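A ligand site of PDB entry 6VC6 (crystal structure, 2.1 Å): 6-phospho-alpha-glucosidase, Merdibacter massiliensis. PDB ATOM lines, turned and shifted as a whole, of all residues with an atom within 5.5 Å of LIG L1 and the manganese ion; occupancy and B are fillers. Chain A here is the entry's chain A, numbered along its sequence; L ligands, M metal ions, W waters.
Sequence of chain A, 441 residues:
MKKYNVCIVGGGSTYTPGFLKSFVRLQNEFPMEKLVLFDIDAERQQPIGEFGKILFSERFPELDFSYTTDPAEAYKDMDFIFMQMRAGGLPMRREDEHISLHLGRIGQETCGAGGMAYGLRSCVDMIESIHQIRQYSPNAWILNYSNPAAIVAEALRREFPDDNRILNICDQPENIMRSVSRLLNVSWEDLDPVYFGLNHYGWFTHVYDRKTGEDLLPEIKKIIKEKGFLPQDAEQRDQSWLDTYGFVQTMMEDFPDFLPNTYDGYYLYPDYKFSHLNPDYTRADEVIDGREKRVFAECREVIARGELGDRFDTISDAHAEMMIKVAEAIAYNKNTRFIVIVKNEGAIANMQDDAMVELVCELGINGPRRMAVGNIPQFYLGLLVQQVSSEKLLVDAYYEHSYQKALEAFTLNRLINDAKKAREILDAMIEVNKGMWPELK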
ATOM      1  N   TYR A  15      22.313  18.631 -12.808  1.00  0.00           N
ATOM      2  CA  TYR A  15      22.280  18.430 -14.240  1.00  0.00           C
ATOM      3  C   TYR A  15      23.358  19.210 -14.982  1.00  0.00           C
ATOM      4  O   TYR A  15      23.604  18.931 -16.161  1.00  0.00           O
ATOM      5  CB  TYR A  15      20.914  18.807 -14.812  1.00  0.00           C
ATOM      6  CG  TYR A  15      19.762  17.957 -14.324  1.00  0.00           C
ATOM      7  CD1 TYR A  15      19.505  16.721 -14.886  1.00  0.00           C
ATOM      8  CD2 TYR A  15      18.932  18.401 -13.305  1.00  0.00           C
ATOM      9  CE1 TYR A  15      18.449  15.934 -14.448  1.00  0.00           C
ATOM     10  CE2 TYR A  15      17.876  17.631 -12.849  1.00  0.00           C
ATOM     11  CZ  TYR A  15      17.643  16.405 -13.431  1.00  0.00           C
ATOM     12  OH  TYR A  15      16.593  15.625 -12.988  1.00  0.00           O
ATOM     13  N   ARG A  86      16.247  25.597  -9.004  1.00  0.00           N
ATOM     14  CA  ARG A  86      15.258  24.962  -8.136  1.00  0.00           C
ATOM     15  C   ARG A  86      15.058  25.889  -6.943  1.00  0.00           C
ATOM     16  O   ARG A  86      15.857  25.865  -5.995  1.00  0.00           O
ATOM     17  CB  ARG A  86      15.694  23.566  -7.707  1.00  0.00           C
ATOM     18  CG  ARG A  86      14.650  22.824  -6.891  1.00  0.00           C
ATOM     19  CD  ARG A  86      15.183  21.499  -6.359  1.00  0.00           C
ATOM     20  NE  ARG A  86      15.352  20.497  -7.409  1.00  0.00           N
ATOM     21  CZ  ARG A  86      14.357  19.752  -7.906  1.00  0.00           C
ATOM     22  NH1 ARG A  86      14.599  18.871  -8.858  1.00  0.00           N
ATOM     23  NH2 ARG A  86      13.127  19.900  -7.434  1.00  0.00           N
ATOM     24  N   ARG A  93      12.126  20.765  -1.541  1.00  0.00           N
ATOM     25  CA  ARG A  93      11.403  19.675  -2.195  1.00  0.00           C
ATOM     26  C   ARG A  93      11.083  18.578  -1.193  1.00  0.00           C
ATOM     27  O   ARG A  93      10.018  17.947  -1.266  1.00  0.00           O
ATOM     28  CB  ARG A  93      12.215  19.121  -3.366  1.00  0.00           C
ATOM     29  CG  ARG A  93      11.538  17.963  -4.093  1.00  0.00           C
ATOM     30  CD  ARG A  93      12.428  17.376  -5.173  1.00  0.00           C
ATOM     31  NE  ARG A  93      11.758  16.318  -5.930  1.00  0.00           N
ATOM     32  CZ  ARG A  93      12.292  15.670  -6.956  1.00  0.00           C
ATOM     33  NH1 ARG A  93      13.517  15.973  -7.359  1.00  0.00           N
ATOM     34  NH2 ARG A  93      11.599  14.734  -7.576  1.00  0.00           N
ATOM     35  N   GLU A 109       6.947  16.455  -6.687  1.00  0.00           N
ATOM     36  CA  GLU A 109       7.719  17.645  -7.021  1.00  0.00           C
ATOM     37  C   GLU A 109       6.862  18.705  -7.710  1.00  0.00           C
ATOM     38  O   GLU A 109       6.907  19.886  -7.341  1.00  0.00           O
ATOM     39  CB  GLU A 109       8.914  17.259  -7.894  1.00  0.00           C
ATOM     40  CG  GLU A 109       9.782  18.440  -8.317  1.00  0.00           C
ATOM     41  CD  GLU A 109      10.551  18.163  -9.601  1.00  0.00           C
ATOM     42  OE1 GLU A 109       9.972  17.524 -10.511  1.00  0.00           O
ATOM     43  OE2 GLU A 109      11.726  18.570  -9.689  1.00  0.00           O
ATOM     44  N   THR A 110       6.094  18.310  -8.717  1.00  0.00           N
ATOM     45  CA  THR A 110       5.356  19.257  -9.533  1.00  0.00           C
ATOM     46  C   THR A 110       3.847  19.067  -9.511  1.00  0.00           C
ATOM     47  O   THR A 110       3.134  19.911 -10.078  1.00  0.00           O
ATOM     48  CB  THR A 110       5.833  19.197 -10.991  1.00  0.00           C
ATOM     49  OG1 THR A 110       5.629  17.876 -11.503  1.00  0.00           O
ATOM     50  CG2 THR A 110       7.311  19.543 -11.084  1.00  0.00           C
ATOM     51  N   ASN A 147      11.110  24.072 -12.922  1.00  0.00           N
ATOM     52  CA  ASN A 147       9.770  23.622 -12.553  1.00  0.00           C
ATOM     53  C   ASN A 147       9.144  24.418 -11.398  1.00  0.00           C
ATOM     54  O   ASN A 147       9.865  25.128 -10.722  1.00  0.00           O
ATOM     55  CB  ASN A 147       9.779  22.133 -12.217  1.00  0.00           C
ATOM     56  CG  ASN A 147       9.555  21.257 -13.427  1.00  0.00           C
ATOM     57  OD1 ASN A 147       8.617  21.477 -14.181  1.00  0.00           O
ATOM     58  ND2 ASN A 147      10.405  20.279 -13.620  1.00  0.00           N
ATOM     59  N   ILE A 169      10.021  24.427 -21.579  1.00  0.00           N
ATOM     60  CA  ILE A 169      10.036  23.105 -22.180  1.00  0.00           C
ATOM     61  C   ILE A 169      10.120  22.039 -21.094  1.00  0.00           C
ATOM     62  O   ILE A 169      10.519  22.305 -19.961  1.00  0.00           O
ATOM     63  CB  ILE A 169      11.209  22.924 -23.184  1.00  0.00           C
ATOM     64  CG1 ILE A 169      12.551  23.036 -22.456  1.00  0.00           C
ATOM     65  CG2 ILE A 169      11.123  23.948 -24.309  1.00  0.00           C
ATOM     66  CD1 ILE A 169      13.719  23.309 -23.377  1.00  0.00           C
ATOM     67  N   CYS A 170       9.734  20.822 -21.464  1.00  0.00           N
ATOM     68  CA  CYS A 170       9.781  19.660 -20.590  1.00  0.00           C
ATOM     69  C   CYS A 170      10.231  18.452 -21.408  1.00  0.00           C
ATOM     70  O   CYS A 170       9.846  18.309 -22.571  1.00  0.00           O
ATOM     71  CB  CYS A 170       8.418  19.370 -19.955  1.00  0.00           C
ATOM     72  SG  CYS A 170       8.329  17.830 -19.025  1.00  0.00           S
ATOM     73  N   ASP A 171      11.037  17.588 -20.786  1.00  0.00           N
ATOM     74  CA  ASP A 171      11.591  16.446 -21.501  1.00  0.00           C
ATOM     75  C   ASP A 171      10.766  15.176 -21.345  1.00  0.00           C
ATOM     76  O   ASP A 171      11.146  14.137 -21.880  1.00  0.00           O
ATOM     77  CB  ASP A 171      13.039  16.181 -21.036  1.00  0.00           C
ATOM     78  CG  ASP A 171      13.141  15.840 -19.564  1.00  0.00           C
ATOM     79  OD1 ASP A 171      14.263  15.540 -19.115  1.00  0.00           O
ATOM     80  OD2 ASP A 171      12.111  15.875 -18.849  1.00  0.00           O
ATOM     81  N   GLN A 172       9.622  15.246 -20.644  1.00  0.00           N
ATOM     82  CA  GLN A 172       8.801  14.048 -20.472  1.00  0.00           C
ATOM     83  C   GLN A 172       8.183  13.565 -21.779  1.00  0.00           C
ATOM     84  O   GLN A 172       8.230  12.354 -22.039  1.00  0.00           O
ATOM     85  CB  GLN A 172       7.736  14.310 -19.392  1.00  0.00           C
ATOM     86  CG  GLN A 172       6.623  13.269 -19.370  1.00  0.00           C
ATOM     87  CD  GLN A 172       7.033  11.979 -18.695  1.00  0.00           C
ATOM     88  OE1 GLN A 172       6.289  11.003 -18.707  1.00  0.00           O
ATOM     89  NE2 GLN A 172       8.208  11.978 -18.080  1.00  0.00           N
ATOM     90  N   ASN A 175      10.897  11.743 -23.629  1.00  0.00           N
ATOM     91  CA  ASN A 175      11.294  10.515 -22.949  1.00  0.00           C
ATOM     92  C   ASN A 175      10.294   9.396 -23.182  1.00  0.00           C
ATOM     93  O   ASN A 175      10.681   8.214 -23.203  1.00  0.00           O
ATOM     94  CB  ASN A 175      11.461  10.782 -21.446  1.00  0.00           C
ATOM     95  CG  ASN A 175      12.782  11.451 -21.122  1.00  0.00           C
ATOM     96  OD1 ASN A 175      13.752  11.322 -21.862  1.00  0.00           O
ATOM     97  ND2 ASN A 175      12.831  12.146 -19.997  1.00  0.00           N
ATOM     98  N   ASN A 199       1.450  20.754 -19.150  1.00  0.00           N
ATOM     99  CA  ASN A 199       2.717  20.149 -18.739  1.00  0.00           C
ATOM    100  C   ASN A 199       2.462  19.116 -17.650  1.00  0.00           C
ATOM    101  O   ASN A 199       1.754  19.366 -16.683  1.00  0.00           O
ATOM    102  CB  ASN A 199       3.682  21.224 -18.238  1.00  0.00           C
ATOM    103  CG  ASN A 199       5.023  20.641 -17.855  1.00  0.00           C
ATOM    104  OD1 ASN A 199       5.728  20.092 -18.690  1.00  0.00           O
ATOM    105  ND2 ASN A 199       5.376  20.747 -16.582  1.00  0.00           N
ATOM    106  N   HIS A 200       3.051  17.929 -17.838  1.00  0.00           N
ATOM    107  CA  HIS A 200       2.881  16.795 -16.921  1.00  0.00           C
ATOM    108  C   HIS A 200       1.411  16.418 -16.790  1.00  0.00           C
ATOM    109  O   HIS A 200       0.935  16.048 -15.718  1.00  0.00           O
ATOM    110  CB  HIS A 200       3.486  17.100 -15.547  1.00  0.00           C
ATOM    111  CG  HIS A 200       4.979  17.252 -15.577  1.00  0.00           C
ATOM    112  ND1 HIS A 200       5.691  17.865 -14.562  1.00  0.00           N
ATOM    113  CD2 HIS A 200       5.884  16.886 -16.501  1.00  0.00           C
ATOM    114  CE1 HIS A 200       6.967  17.850 -14.863  1.00  0.00           C
ATOM    115  NE2 HIS A 200       7.126  17.260 -16.031  1.00  0.00           N
ATOM    116  N   TRP A 241      11.167   5.199 -10.671  1.00  0.00           N
ATOM    117  CA  TRP A 241      10.906   5.550 -12.071  1.00  0.00           C
ATOM    118  C   TRP A 241      10.453   4.336 -12.871  1.00  0.00           C
ATOM    119  O   TRP A 241       9.630   4.464 -13.780  1.00  0.00           O
ATOM    120  CB  TRP A 241      12.147   6.185 -12.691  1.00  0.00           C
ATOM    121  CG  TRP A 241      12.187   7.680 -12.589  1.00  0.00           C
ATOM    122  CD1 TRP A 241      13.138   8.438 -11.980  1.00  0.00           C
ATOM    123  CD2 TRP A 241      11.209   8.592 -13.097  1.00  0.00           C
ATOM    124  NE1 TRP A 241      12.825   9.769 -12.092  1.00  0.00           N
ATOM    125  CE2 TRP A 241      11.646   9.896 -12.766  1.00  0.00           C
ATOM    126  CE3 TRP A 241      10.009   8.450 -13.809  1.00  0.00           C
ATOM    127  CZ2 TRP A 241      10.927  11.039 -13.122  1.00  0.00           C
ATOM    128  CZ3 TRP A 241       9.300   9.590 -14.151  1.00  0.00           C
ATOM    129  CH2 TRP A 241       9.758  10.860 -13.811  1.00  0.00           C
ATOM    130  N   TYR A 263       2.829  11.221 -15.961  1.00  0.00           N
ATOM    131  CA  TYR A 263       2.300  11.986 -14.843  1.00  0.00           C
ATOM    132  C   TYR A 263       0.782  11.896 -14.732  1.00  0.00           C
ATOM    133  O   TYR A 263       0.225  12.309 -13.708  1.00  0.00           O
ATOM    134  CB  TYR A 263       2.723  13.453 -14.964  1.00  0.00           C
ATOM    135  CG  TYR A 263       4.128  13.712 -14.477  1.00  0.00           C
ATOM    136  CD1 TYR A 263       4.402  13.831 -13.119  1.00  0.00           C
ATOM    137  CD2 TYR A 263       5.185  13.790 -15.368  1.00  0.00           C
ATOM    138  CE1 TYR A 263       5.686  14.062 -12.671  1.00  0.00           C
ATOM    139  CE2 TYR A 263       6.473  14.025 -14.929  1.00  0.00           C
ATOM    140  CZ  TYR A 263       6.719  14.156 -13.578  1.00  0.00           C
ATOM    141  OH  TYR A 263       8.003  14.388 -13.131  1.00  0.00           O
ATOM    142  N   ARG A 283      11.052  10.914  -2.697  1.00  0.00           N
ATOM    143  CA  ARG A 283      11.864  10.990  -3.902  1.00  0.00           C
ATOM    144  C   ARG A 283      12.987  12.007  -3.756  1.00  0.00           C
ATOM    145  O   ARG A 283      14.091  11.822  -4.286  1.00  0.00           O
ATOM    146  CB  ARG A 283      10.983  11.331  -5.105  1.00  0.00           C
ATOM    147  CG  ARG A 283      11.732  11.550  -6.412  1.00  0.00           C
ATOM    148  CD  ARG A 283      12.558  10.332  -6.806  1.00  0.00           C
ATOM    149  NE  ARG A 283      13.368  10.598  -8.001  1.00  0.00           N
ATOM    150  CZ  ARG A 283      14.321   9.799  -8.440  1.00  0.00           C
ATOM    151  NH1 ARG A 283      14.597   8.671  -7.799  1.00  0.00           N
ATOM    152  NH2 ARG A 283      15.004  10.117  -9.533  1.00  0.00           N
ATOM    153  N   VAL A 287      16.896  11.366  -4.530  1.00  0.00           N
ATOM    154  CA  VAL A 287      17.785  12.193  -5.325  1.00  0.00           C
ATOM    155  C   VAL A 287      18.987  12.626  -4.506  1.00  0.00           C
ATOM    156  O   VAL A 287      20.130  12.608  -4.993  1.00  0.00           O
ATOM    157  CB  VAL A 287      17.025  13.409  -5.892  1.00  0.00           C
ATOM    158  CG1 VAL A 287      18.003  14.360  -6.592  1.00  0.00           C
ATOM    159  CG2 VAL A 287      15.942  12.955  -6.850  1.00  0.00           C
ATOM    160  N   ARG A 291      21.325  10.816  -7.321  1.00  0.00           N
ATOM    161  CA  ARG A 291      21.912  11.625  -8.392  1.00  0.00           C
ATOM    162  C   ARG A 291      22.808  12.723  -7.809  1.00  0.00           C
ATOM    163  O   ARG A 291      23.916  12.959  -8.322  1.00  0.00           O
ATOM    164  CB  ARG A 291      20.812  12.246  -9.254  1.00  0.00           C
ATOM    165  CG  ARG A 291      21.241  13.505  -9.989  1.00  0.00           C
ATOM    166  CD  ARG A 291      20.232  13.903 -11.054  1.00  0.00           C
ATOM    167  NE  ARG A 291      19.214  14.813 -10.522  1.00  0.00           N
ATOM    168  CZ  ARG A 291      17.940  14.476 -10.348  1.00  0.00           C
ATOM    169  NH1 ARG A 291      17.518  13.257 -10.654  1.00  0.00           N
ATOM    170  NH2 ARG A 291      17.090  15.363  -9.855  1.00  0.00           N
HETATM  171  C1  LIG L   1      10.403  14.146 -15.209  1.00  0.00           C
HETATM  172  C2  LIG L   1       9.939  15.571 -15.548  1.00  0.00           C
HETATM  173  C3  LIG L   1      10.665  16.665 -14.799  1.00  0.00           C
HETATM  174  C4  LIG L   1      10.843  16.235 -13.360  1.00  0.00           C
HETATM  175  C5  LIG L   1      11.826  15.070 -13.356  1.00  0.00           C
HETATM  176  C6  LIG L   1      11.950  14.524 -11.938  1.00  0.00           C
HETATM  177  O1  LIG L   1      10.824  13.473 -16.409  1.00  0.00           O
HETATM  178  O2  LIG L   1      10.097  15.796 -16.961  1.00  0.00           O
HETATM  179  O3  LIG L   1       9.932  17.889 -14.845  1.00  0.00           O
HETATM  180  O4  LIG L   1      11.376  17.318 -12.596  1.00  0.00           O
HETATM  181  O5  LIG L   1      11.420  13.988 -14.192  1.00  0.00           O
HETATM  182  O6  LIG L   1      13.223  13.895 -11.808  1.00  0.00           O
HETATM  183  P1  LIG L   1      13.783  13.489 -10.355  1.00  0.00           P
HETATM  184  O7  LIG L   1      14.414  14.772  -9.867  1.00  0.00           O
HETATM  185  O8  LIG L   1      12.560  13.061  -9.583  1.00  0.00           O
HETATM  186  O9  LIG L   1      14.743  12.359 -10.648  1.00  0.00           O
HETATM  187  P1  LG2 L   2      19.329  21.210  -7.718  1.00  0.00           P
HETATM  188  O1  LG2 L   2      20.386  20.134  -7.822  1.00  0.00           O
HETATM  189  O2  LG2 L   2      18.899  21.709  -6.355  1.00  0.00           O
HETATM  190  O3  LG2 L   2      19.789  22.468  -8.589  1.00  0.00           O
HETATM  191  C1  LG2 L   2      19.166  23.736  -8.422  1.00  0.00           C
HETATM  192  C2  LG2 L   2      20.211  24.841  -8.507  1.00  0.00           C
HETATM  193  O4  LG2 L   2      19.571  26.094  -8.778  1.00  0.00           O
HETATM  194  C3  LG2 L   2      20.956  24.973  -7.192  1.00  0.00           C
HETATM  195  O5  LG2 L   2      22.366  24.939  -7.442  1.00  0.00           O
HETATM  196  C4  LG2 L   2      20.570  26.339  -6.656  1.00  0.00           C
HETATM  197  O6  LG2 L   2      21.694  26.974  -6.051  1.00  0.00           O
HETATM  198  C5  LG2 L   2      20.116  27.085  -7.893  1.00  0.00           C
HETATM  199  N1  LG2 L   2      19.117  28.125  -7.570  1.00  0.00           N
HETATM  200  C6  LG2 L   2      18.078  28.016  -6.717  1.00  0.00           C
HETATM  201  N2  LG2 L   2      17.366  29.171  -6.664  1.00  0.00           N
HETATM  202  C7  LG2 L   2      17.965  30.050  -7.497  1.00  0.00           C
HETATM  203  C8  LG2 L   2      17.741  31.453  -7.912  1.00  0.00           C
HETATM  204  N3  LG2 L   2      16.706  32.178  -7.420  1.00  0.00           N
HETATM  205  N4  LG2 L   2      18.603  31.990  -8.813  1.00  0.00           N
HETATM  206  C9  LG2 L   2      19.638  31.282  -9.310  1.00  0.00           C
HETATM  207  N5  LG2 L   2      19.895  30.018  -8.968  1.00  0.00           N
HETATM  208  C10 LG2 L   2      19.110  29.350  -8.081  1.00  0.00           C
HETATM  209  O7  LG2 L   2      18.013  20.736  -8.521  1.00  0.00           O
HETATM  210  P2  LG2 L   2      18.065  19.633  -9.693  1.00  0.00           P
HETATM  211  O8  LG2 L   2      17.531  18.325  -9.148  1.00  0.00           O
HETATM  212  O9  LG2 L   2      19.407  19.696 -10.385  1.00  0.00           O
HETATM  213  O10 LG2 L   2      16.960  20.260 -10.682  1.00  0.00           O
HETATM  214  C11 LG2 L   2      17.290  21.346 -11.534  1.00  0.00           C
HETATM  215  C12 LG2 L   2      16.002  21.931 -12.100  1.00  0.00           C
HETATM  216  O11 LG2 L   2      15.723  21.344 -13.367  1.00  0.00           O
HETATM  217  C13 LG2 L   2      14.823  21.597 -11.183  1.00  0.00           C
HETATM  218  O12 LG2 L   2      14.050  22.783 -10.984  1.00  0.00           O
HETATM  219  C14 LG2 L   2      14.001  20.601 -11.972  1.00  0.00           C
HETATM  220  O13 LG2 L   2      12.605  20.767 -11.703  1.00  0.00           O
HETATM  221  C15 LG2 L   2      14.341  20.984 -13.397  1.00  0.00           C
HETATM  222  N6  LG2 L   2      14.064  19.913 -14.345  1.00  0.00           N
HETATM  223  C16 LG2 L   2      13.075  20.128 -15.226  1.00  0.00           C
HETATM  224  C17 LG2 L   2      12.742  19.164 -16.170  1.00  0.00           C
HETATM  225  C18 LG2 L   2      11.628  19.468 -17.131  1.00  0.00           C
HETATM  226  O14 LG2 L   2      11.160  18.559 -17.804  1.00  0.00           O
HETATM  227  N7  LG2 L   2      11.178  20.713 -17.219  1.00  0.00           N
HETATM  228  C19 LG2 L   2      13.444  17.969 -16.196  1.00  0.00           C
HETATM  229  C20 LG2 L   2      14.450  17.767 -15.269  1.00  0.00           C
HETATM  230  C21 LG2 L   2      14.752  18.768 -14.347  1.00  0.00           C
HETATM  231 MN    MN M   1       8.944  18.043 -16.944  1.00  0.00          MN
HETATM  232  O   HOH W   1      15.008  12.401 -14.104  1.00  0.00           O
HETATM  233  O   HOH W   2      10.356  11.294  -9.818  1.00  0.00           O
HETATM  234  O   HOH W   3      14.197  17.012 -11.503  1.00  0.00           O
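Within 4 Å of the manganese ion: Cys 170 and His 200. The nearest printed residue that does not touch the manganese ion is Asn 199 (4.2 Å).
The guanidinium group of Arg 283 lies within salt-bridge range of an oxygen (O9) of LIG L1, 2.5 Å away. The side-chain carboxylate (OE1) of Glu 109 is in hydrogen-bond range of an oxygen (O4) of LIG L1, at 2.5 Å. ND2 of Asn 147 lies within hydrogen-bond range of O4 of LIG L1 (3.3 Å). The guanidinium group (NH2) of Arg 291 is in salt-bridge range of an oxygen (O7) of LIG L1. An oxygen (O2) of LIG L1 sits close to the side-chain carboxylate (OD2) of Asp 171, at 2.8 Å. An oxygen (O8) of LIG L1 is in salt-bridge range of the guanidinium group of Arg 93. The side-chain amide nitrogen (NE2) of Gln 172 sits at hydrogen-bond distance from an oxygen (O1) of LIG L1. The side-chain carboxylate of Glu 109 is in hydrogen-bond range of an oxygen (O13) of LG2 L2 (3.1 Å). The side-chain amide nitrogen (ND2) of Asn 147 lies within hydrogen-bond range of an oxygen (O13) of LG2 L2. The guanidinium group (NH2) of Arg 291 lies within salt-bridge range of an oxygen (O8) of LG2 L2 (3.1 Å). O14 of LG2 L2 lies close to N of Asp 171, at 3.1 Å. An oxygen (O4) of LG2 L2 sits at hydrogen-bond distance from the backbone NH (N) of Arg 86 (3.4 Å). The guanidinium group of Arg 86 lies within salt-bridge range of an oxygen (O8) of LG2 L2 (3.0 Å). N7 of LG2 L2 is in hydrogen-bond range of O of Ile 169 (3.2 Å).
The manganese ion is bound by NE2 of His 200 (2.2 Å). The side-chain sulfur (SG) of Cys 170 is bound to the manganese ion, at 2.2 Å. An oxygen (O3) of LIG L1 binds the manganese ion (2.3 Å). The manganese ion is bound by an oxygen (O14) of LG2 L2 (2.4 Å). The manganese ion is bound by O2 of LIG L1, 2.5 Å away.
Tyr 15 touches LIG L1 (OH to O7, 3.9 Å). CZ2 of Trp 241 touches O5 of LIG L1, at 3.2 Å. Tyr 263 touches LIG L1. Val 287 touches LIG L1 (CG2 to O7, 3.8 Å). Hydrophobic or aromatic side chains within 4 Å of LIG L1: His 200, Trp 241, Tyr 263 and Val 287. Along chain A the residues within 4 Å of LIG L1 span positions 15 to 291.
OG1 of Thr 110 sits at hydrogen-bond distance from ND1 of His 200 (3.1 Å). N of Gln 172 lies close to SG of Cys 170 (3.3 Å). The side-chain sulfur of Cys 170 sits close to the side-chain amide oxygen of Asn 199 (3.5 Å). The guanidinium group of Arg 93 is in salt-bridge range of the side-chain carboxylate of Glu 109, at 3.9 Å. The side-chain carboxylate (OE2) of Glu 109 lies within salt-bridge range of the guanidinium group (NH2) of Arg 86 (3.0 Å). NH2 of Arg 291 sits close to OH of Tyr 15 (3.2 Å). O of Asp 171 lies within hydrogen-bond range of ND2 of Asn 175 (3.2 Å).
Water W3 lies within hydrogen-bond range of an oxygen (O7) of LIG L1 (2.8 Å), the side-chain hydroxyl (OH) of Tyr 15 (3.1 Å), the guanidinium group (NH1) of Arg 86 (3.3 Å) and the side-chain carboxylate (OE2) of Glu 109 (3.4 Å).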
